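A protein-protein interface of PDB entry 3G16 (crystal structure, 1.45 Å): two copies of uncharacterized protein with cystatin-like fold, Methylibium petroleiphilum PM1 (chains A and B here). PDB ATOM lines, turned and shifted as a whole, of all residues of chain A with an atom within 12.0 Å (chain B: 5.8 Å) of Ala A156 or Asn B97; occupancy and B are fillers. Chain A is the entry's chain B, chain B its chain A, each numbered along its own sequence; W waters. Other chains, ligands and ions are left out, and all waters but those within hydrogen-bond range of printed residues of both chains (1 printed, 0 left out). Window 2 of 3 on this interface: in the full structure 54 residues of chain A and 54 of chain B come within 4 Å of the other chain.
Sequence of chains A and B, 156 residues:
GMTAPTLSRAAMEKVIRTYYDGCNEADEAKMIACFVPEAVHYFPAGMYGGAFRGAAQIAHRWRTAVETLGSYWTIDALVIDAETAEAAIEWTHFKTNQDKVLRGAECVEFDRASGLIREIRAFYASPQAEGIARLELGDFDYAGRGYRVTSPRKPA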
ATOM      1  N   ILE A 132     -10.682   0.509 -21.836  1.00  0.00           N
ATOM      2  CA  ILE A 132     -11.003  -0.645 -21.029  1.00  0.00           C
ATOM      3  C   ILE A 132     -12.493  -0.555 -20.679  1.00  0.00           C
ATOM      4  O   ILE A 132     -12.938   0.399 -20.051  1.00  0.00           O
ATOM      5  CB  ILE A 132     -10.180  -0.685 -19.742  1.00  0.00           C
ATOM      6  CG1 ILE A 132      -8.660  -0.681 -20.040  1.00  0.00           C
ATOM      7  CG2 ILE A 132     -10.580  -1.892 -18.910  1.00  0.00           C
ATOM      8  CD1 ILE A 132      -8.235  -1.839 -20.849  1.00  0.00           C
ATOM      9  N   ALA A 133     -13.261  -1.555 -21.071  1.00  0.00           N
ATOM     10  CA  ALA A 133     -14.711  -1.499 -20.892  1.00  0.00           C
ATOM     11  C   ALA A 133     -15.152  -1.644 -19.447  1.00  0.00           C
ATOM     12  O   ALA A 133     -16.154  -1.046 -19.054  1.00  0.00           O
ATOM     13  CB  ALA A 133     -15.383  -2.585 -21.750  1.00  0.00           C
ATOM     14  N   ARG A 134     -14.451  -2.473 -18.681  1.00  0.00           N
ATOM     15  CA  ARG A 134     -14.826  -2.750 -17.304  1.00  0.00           C
ATOM     16  C   ARG A 134     -13.623  -2.496 -16.392  1.00  0.00           C
ATOM     17  O   ARG A 134     -12.638  -3.217 -16.436  1.00  0.00           O
ATOM     18  CB  ARG A 134     -15.354  -4.193 -17.132  1.00  0.00           C
ATOM     19  CG  ARG A 134     -16.475  -4.605 -18.082  1.00  0.00           C
ATOM     20  CD  ARG A 134     -17.134  -5.949 -17.676  1.00  0.00           C
ATOM     21  NE  ARG A 134     -17.765  -5.886 -16.357  1.00  0.00           N
ATOM     22  CZ  ARG A 134     -19.025  -5.545 -16.087  1.00  0.00           C
ATOM     23  NH1 ARG A 134     -19.906  -5.278 -17.045  1.00  0.00           N
ATOM     24  NH2 ARG A 134     -19.406  -5.496 -14.801  1.00  0.00           N
ATOM     25  N   VAL A 149     -23.949  -6.170 -12.358  1.00  0.00           N
ATOM     26  CA  VAL A 149     -22.961  -6.298 -13.392  1.00  0.00           C
ATOM     27  C   VAL A 149     -23.335  -5.544 -14.657  1.00  0.00           C
ATOM     28  O   VAL A 149     -22.488  -5.251 -15.459  1.00  0.00           O
ATOM     29  CB  VAL A 149     -22.739  -7.783 -13.651  1.00  0.00           C
ATOM     30  CG1 VAL A 149     -22.162  -8.039 -15.008  1.00  0.00           C
ATOM     31  CG2 VAL A 149     -21.873  -8.370 -12.517  1.00  0.00           C
ATOM     32  N   THR A 150     -24.610  -5.233 -14.831  1.00  0.00           N
ATOM     33  CA  THR A 150     -25.125  -4.525 -15.984  1.00  0.00           C
ATOM     34  C   THR A 150     -25.873  -3.298 -15.484  1.00  0.00           C
ATOM     35  O   THR A 150     -26.574  -3.354 -14.440  1.00  0.00           O
ATOM     36  CB  THR A 150     -26.069  -5.408 -16.786  1.00  0.00           C
ATOM     37  OG1 THR A 150     -25.358  -6.606 -17.174  1.00  0.00           O
ATOM     38  CG2 THR A 150     -26.560  -4.691 -18.042  1.00  0.00           C
ATOM     39  N   SER A 151     -25.770  -2.174 -16.200  1.00  0.00           N
ATOM     40  CA  SER A 151     -26.438  -0.976 -15.752  1.00  0.00           C
ATOM     41  C   SER A 151     -27.964  -1.209 -15.613  1.00  0.00           C
ATOM     42  O   SER A 151     -28.610  -1.771 -16.486  1.00  0.00           O
ATOM     43  CB  SER A 151     -26.304   0.147 -16.780  1.00  0.00           C
ATOM     44  OG  SER A 151     -26.893   1.332 -16.291  1.00  0.00           O
ATOM     45  N   PRO A 152     -28.540  -0.722 -14.485  1.00  0.00           N
ATOM     46  CA  PRO A 152     -29.998  -0.725 -14.357  1.00  0.00           C
ATOM     47  C   PRO A 152     -30.717   0.182 -15.352  1.00  0.00           C
ATOM     48  O   PRO A 152     -31.870  -0.066 -15.625  1.00  0.00           O
ATOM     49  CB  PRO A 152     -30.220  -0.217 -12.923  1.00  0.00           C
ATOM     50  CG  PRO A 152     -28.993  -0.613 -12.211  1.00  0.00           C
ATOM     51  CD  PRO A 152     -27.898  -0.337 -13.212  1.00  0.00           C
ATOM     52  N   ARG A 153     -30.003   1.172 -15.897  1.00  0.00           N
ATOM     53  CA  ARG A 153     -30.650   2.120 -16.775  1.00  0.00           C
ATOM     54  C   ARG A 153     -30.813   1.606 -18.200  1.00  0.00           C
ATOM     55  O   ARG A 153     -29.867   1.072 -18.766  1.00  0.00           O
ATOM     56  CB  ARG A 153     -29.848   3.434 -16.784  1.00  0.00           C
ATOM     57  CG  ARG A 153     -30.625   4.584 -17.424  1.00  0.00           C
ATOM     58  CD  ARG A 153     -29.796   5.849 -17.584  1.00  0.00           C
ATOM     59  NE  ARG A 153     -29.301   6.469 -16.335  1.00  0.00           N
ATOM     60  CZ  ARG A 153     -30.032   7.283 -15.564  1.00  0.00           C
ATOM     61  NH1 ARG A 153     -31.296   7.523 -15.817  1.00  0.00           N
ATOM     62  NH2 ARG A 153     -29.473   7.825 -14.494  1.00  0.00           N
ATOM     63  N   LYS A 154     -31.966   1.837 -18.785  1.00  0.00           N
ATOM     64  CA  LYS A 154     -32.157   1.463 -20.197  1.00  0.00           C
ATOM     65  C   LYS A 154     -31.204   2.291 -21.068  1.00  0.00           C
ATOM     66  O   LYS A 154     -31.106   3.514 -20.895  1.00  0.00           O
ATOM     67  CB  LYS A 154     -33.586   1.713 -20.620  1.00  0.00           C
ATOM     68  CG  LYS A 154     -33.902   1.201 -22.024  1.00  0.00           C
ATOM     69  CD  LYS A 154     -35.331   1.450 -22.304  1.00  0.00           C
ATOM     70  CE  LYS A 154     -35.694   1.033 -23.753  1.00  0.00           C
ATOM     71  NZ  LYS A 154     -37.116   1.300 -24.076  1.00  0.00           N
ATOM     72  N   PRO A 155     -30.418   1.622 -21.945  1.00  0.00           N
ATOM     73  CA  PRO A 155     -29.520   2.401 -22.784  1.00  0.00           C
ATOM     74  C   PRO A 155     -30.299   3.314 -23.750  1.00  0.00           C
ATOM     75  O   PRO A 155     -31.398   2.992 -24.166  1.00  0.00           O
ATOM     76  CB  PRO A 155     -28.714   1.331 -23.557  1.00  0.00           C
ATOM     77  CG  PRO A 155     -28.957   0.048 -22.860  1.00  0.00           C
ATOM     78  CD  PRO A 155     -30.311   0.174 -22.205  1.00  0.00           C
ATOM     79  N   ALA A 156     -29.697   4.459 -24.062  1.00  0.00           N
ATOM     80  CA  ALA A 156     -30.310   5.437 -24.957  1.00  0.00           C
ATOM     81  C   ALA A 156     -30.340   4.862 -26.376  1.00  0.00           C
ATOM     82  O   ALA A 156     -31.323   5.070 -27.109  1.00  0.00           O
ATOM     83  CB  ALA A 156     -29.534   6.742 -24.927  1.00  0.00           C
ATOM     84  OXT ALA A 156     -29.405   4.155 -26.806  1.00  0.00           O
ATOM     85  N   VAL B  66     -25.343  12.194 -16.481  1.00  0.00           N
ATOM     86  CA  VAL B  66     -26.549  11.400 -16.763  1.00  0.00           C
ATOM     87  C   VAL B  66     -27.058  11.657 -18.184  1.00  0.00           C
ATOM     88  O   VAL B  66     -27.401  10.739 -18.933  1.00  0.00           O
ATOM     89  CB  VAL B  66     -27.631  11.682 -15.723  1.00  0.00           C
ATOM     90  CG1 VAL B  66     -29.042  11.114 -16.133  1.00  0.00           C
ATOM     91  CG2 VAL B  66     -27.168  11.153 -14.368  1.00  0.00           C
ATOM     92  N   GLU B  67     -27.080  12.932 -18.568  1.00  0.00           N
ATOM     93  CA  GLU B  67     -27.623  13.299 -19.874  1.00  0.00           C
ATOM     94  C   GLU B  67     -26.797  12.784 -21.002  1.00  0.00           C
ATOM     95  O   GLU B  67     -27.353  12.290 -22.020  1.00  0.00           O
ATOM     96  CB  GLU B  67     -27.729  14.818 -19.997  1.00  0.00           C
ATOM     97  CG  GLU B  67     -28.762  15.393 -19.102  1.00  0.00           C
ATOM     98  CD  GLU B  67     -28.807  16.905 -19.081  1.00  0.00           C
ATOM     99  OE1 GLU B  67     -27.801  17.535 -19.513  1.00  0.00           O
ATOM    100  OE2 GLU B  67     -29.795  17.415 -18.530  1.00  0.00           O
ATOM    101  N   THR B  68     -25.486  12.865 -20.860  1.00  0.00           N
ATOM    102  CA  THR B  68     -24.596  12.513 -21.980  1.00  0.00           C
ATOM    103  C   THR B  68     -24.113  11.076 -21.985  1.00  0.00           C
ATOM    104  O   THR B  68     -23.953  10.477 -23.055  1.00  0.00           O
ATOM    105  CB  THR B  68     -23.377  13.437 -22.023  1.00  0.00           C
ATOM    106  OG1 THR B  68     -22.566  13.223 -20.890  1.00  0.00           O
ATOM    107  CG2 THR B  68     -23.802  14.926 -22.114  1.00  0.00           C
ATOM    108  N   LEU B  69     -23.875  10.507 -20.800  1.00  0.00           N
ATOM    109  CA  LEU B  69     -23.349   9.163 -20.694  1.00  0.00           C
ATOM    110  C   LEU B  69     -24.411   8.127 -20.285  1.00  0.00           C
ATOM    111  O   LEU B  69     -24.162   6.927 -20.384  1.00  0.00           O
ATOM    112  CB  LEU B  69     -22.245   9.109 -19.645  1.00  0.00           C
ATOM    113  CG  LEU B  69     -21.049  10.079 -19.766  1.00  0.00           C
ATOM    114  CD1 LEU B  69     -20.104   9.903 -18.630  1.00  0.00           C
ATOM    115  CD2 LEU B  69     -20.370   9.858 -21.143  1.00  0.00           C
ATOM    116  N   GLY B  70     -25.555   8.582 -19.824  1.00  0.00           N
ATOM    117  CA  GLY B  70     -26.530   7.674 -19.245  1.00  0.00           C
ATOM    118  C   GLY B  70     -26.053   7.134 -17.896  1.00  0.00           C
ATOM    119  O   GLY B  70     -26.493   6.045 -17.462  1.00  0.00           O
ATOM    120  N   SER B  71     -25.164   7.854 -17.207  1.00  0.00           N
ATOM    121  CA  SER B  71     -24.602   7.428 -15.950  1.00  0.00           C
ATOM    122  C   SER B  71     -25.676   6.952 -14.975  1.00  0.00           C
ATOM    123  O   SER B  71     -26.726   7.541 -14.852  1.00  0.00           O
ATOM    124  CB  SER B  71     -23.874   8.564 -15.313  1.00  0.00           C
ATOM    125  OG  SER B  71     -22.777   8.959 -16.125  1.00  0.00           O
ATOM    126  N   LYS B  95     -21.591   3.668 -17.106  1.00  0.00           N
ATOM    127  CA  LYS B  95     -21.647   4.657 -18.199  1.00  0.00           C
ATOM    128  C   LYS B  95     -22.465   3.962 -19.275  1.00  0.00           C
ATOM    129  O   LYS B  95     -21.952   3.477 -20.282  1.00  0.00           O
ATOM    130  CB  LYS B  95     -20.238   5.010 -18.661  1.00  0.00           C
ATOM    131  CG  LYS B  95     -19.461   5.703 -17.590  1.00  0.00           C
ATOM    132  CD  LYS B  95     -18.040   5.806 -18.003  1.00  0.00           C
ATOM    133  CE  LYS B  95     -17.219   6.455 -17.018  1.00  0.00           C
ATOM    134  NZ  LYS B  95     -15.877   6.486 -17.681  1.00  0.00           N
ATOM    135  N   THR B  96     -23.768   3.942 -19.060  1.00  0.00           N
ATOM    136  CA  THR B  96     -24.668   3.118 -19.804  1.00  0.00           C
ATOM    137  C   THR B  96     -24.535   3.242 -21.297  1.00  0.00           C
ATOM    138  O   THR B  96     -24.451   2.226 -22.028  1.00  0.00           O
ATOM    139  CB  THR B  96     -26.132   3.409 -19.372  1.00  0.00           C
ATOM    140  OG1 THR B  96     -26.189   3.416 -17.940  1.00  0.00           O
ATOM    141  CG2 THR B  96     -27.126   2.362 -19.967  1.00  0.00           C
ATOM    142  N   ASN B  97     -24.532   4.494 -21.765  1.00  0.00           N
ATOM    143  CA  ASN B  97     -24.572   4.713 -23.207  1.00  0.00           C
ATOM    144  C   ASN B  97     -23.258   4.395 -23.903  1.00  0.00           C
ATOM    145  O   ASN B  97     -23.241   4.301 -25.137  1.00  0.00           O
ATOM    146  CB  ASN B  97     -25.001   6.141 -23.490  1.00  0.00           C
ATOM    147  CG  ASN B  97     -26.403   6.452 -22.998  1.00  0.00           C
ATOM    148  OD1 ASN B  97     -27.209   5.569 -22.691  1.00  0.00           O
ATOM    149  ND2 ASN B  97     -26.677   7.746 -22.896  1.00  0.00           N
ATOM    150  N   GLN B  98     -22.203   4.221 -23.148  1.00  0.00           N
ATOM    151  CA  GLN B  98     -20.880   3.813 -23.671  1.00  0.00           C
ATOM    152  C   GLN B  98     -20.620   2.321 -23.453  1.00  0.00           C
ATOM    153  O   GLN B  98     -19.570   1.800 -23.883  1.00  0.00           O
ATOM    154  CB  GLN B  98     -19.771   4.584 -22.972  1.00  0.00           C
ATOM    155  CG  GLN B  98     -19.823   6.068 -23.257  1.00  0.00           C
ATOM    156  CD  GLN B  98     -18.740   6.814 -22.542  1.00  0.00           C
ATOM    157  OE1 GLN B  98     -18.272   6.413 -21.460  1.00  0.00           O
ATOM    158  NE2 GLN B  98     -18.332   7.950 -23.128  1.00  0.00           N
ATOM    159  N   ASP B  99     -21.540   1.631 -22.784  1.00  0.00           N
ATOM    160  CA  ASP B  99     -21.381   0.262 -22.394  1.00  0.00           C
ATOM    161  C   ASP B  99     -20.060   0.075 -21.626  1.00  0.00           C
ATOM    162  O   ASP B  99     -19.299  -0.865 -21.875  1.00  0.00           O
ATOM    163  CB  ASP B  99     -21.428  -0.680 -23.613  1.00  0.00           C
ATOM    164  CG  ASP B  99     -21.694  -2.126 -23.217  1.00  0.00           C
ATOM    165  OD1 ASP B  99     -22.402  -2.349 -22.197  1.00  0.00           O
ATOM    166  OD2 ASP B  99     -21.226  -3.030 -23.946  1.00  0.00           O
HETATM  167  O   HOH W   1     -29.144   5.514 -20.759  1.00  0.00           O
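Among the printed residues, pairs that only touch across the chains: Arg A153 with Val B66, Arg A153 with Thr B96, Pro A155 with Thr B96 and Pro A155 with Asn B97.
Ala A156 touches just one residue of chain B: Asn B97.
Asn B97 touches just these residues of chain A: Pro A155 and Ala A156.
No residue of chain A comes within 4 Å of Thr B68.
No residue of chain A comes within 4 Å of Leu B69.
No residue of chain A comes within 4 Å of Gln B98.
No residue of chain A comes within 4 Å of Asp B99.
Printed residues of chain B within 4 Å of Arg A153: Val B66, Gly B70, Ser B71 and Thr B96.
Printed residues of chain B within 4 Å of Ser A151: Thr B96.
Ile A132 touches none of the printed residues of chain B.
Thr A150 touches none of the printed residues of chain B.
The nearest residue of chain B that does not touch Ala A156 is Thr B96 (5.3 Å).
The nearest residue of chain A that does not touch Asn B97 is Lys A154 (4.8 Å).
No position is printed for both chains.
Of the 8 pairs that touch across the chains among the printed residues, none has its exchanged pair printed and touching as well.
Printed residues of chain B that touch a printed residue of chain A: Val B66, Gly B70, Ser B71, Thr B96 and Asn B97.
Printed residues of chain A that touch a printed residue of chain B: Ser A151, Arg A153, Pro A155 and Ala A156.
Water W1 lies within hydrogen-bond range of OD1 of Asn B97 (2.7 Å) and O of Lys A154 (2.8 Å).
The guanidinium group of Arg A153 lies within hydrogen-bond range of the backbone carbonyl oxygen of Gly B70 (3.1 Å).
OD1 of Asn B97 lies within hydrogen-bond range of N of Ala A156, at 3.0 Å.
OG1 of Thr B96 lies within hydrogen-bond range of OG of Ser A151 (2.7 Å).
The backbone carbonyl oxygen (O) of Ser B71 sits at hydrogen-bond distance from the guanidinium group (NH2) of Arg A153, 2.8 Å away.
The backbone carbonyl oxygen of Gly B70 lies within hydrogen-bond range of the side-chain hydroxyl of Thr B96, at 2.7 Å.
The backbone NH of Thr B96 is in hydrogen-bond range of the backbone carbonyl oxygen of Leu B69.
The backbone NH (N) of Gly B70 lies close to the side-chain amide nitrogen (ND2) of Asn B97 (3.4 Å).
The backbone carbonyl oxygen (O) of Leu B69 is in hydrogen-bond range of the backbone NH (N) of Asn B97 (2.8 Å).
The side-chain hydroxyl (OG) of Ser A151 lies within hydrogen-bond range of the backbone NH (N) of Arg A153, 3.1 Å away.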
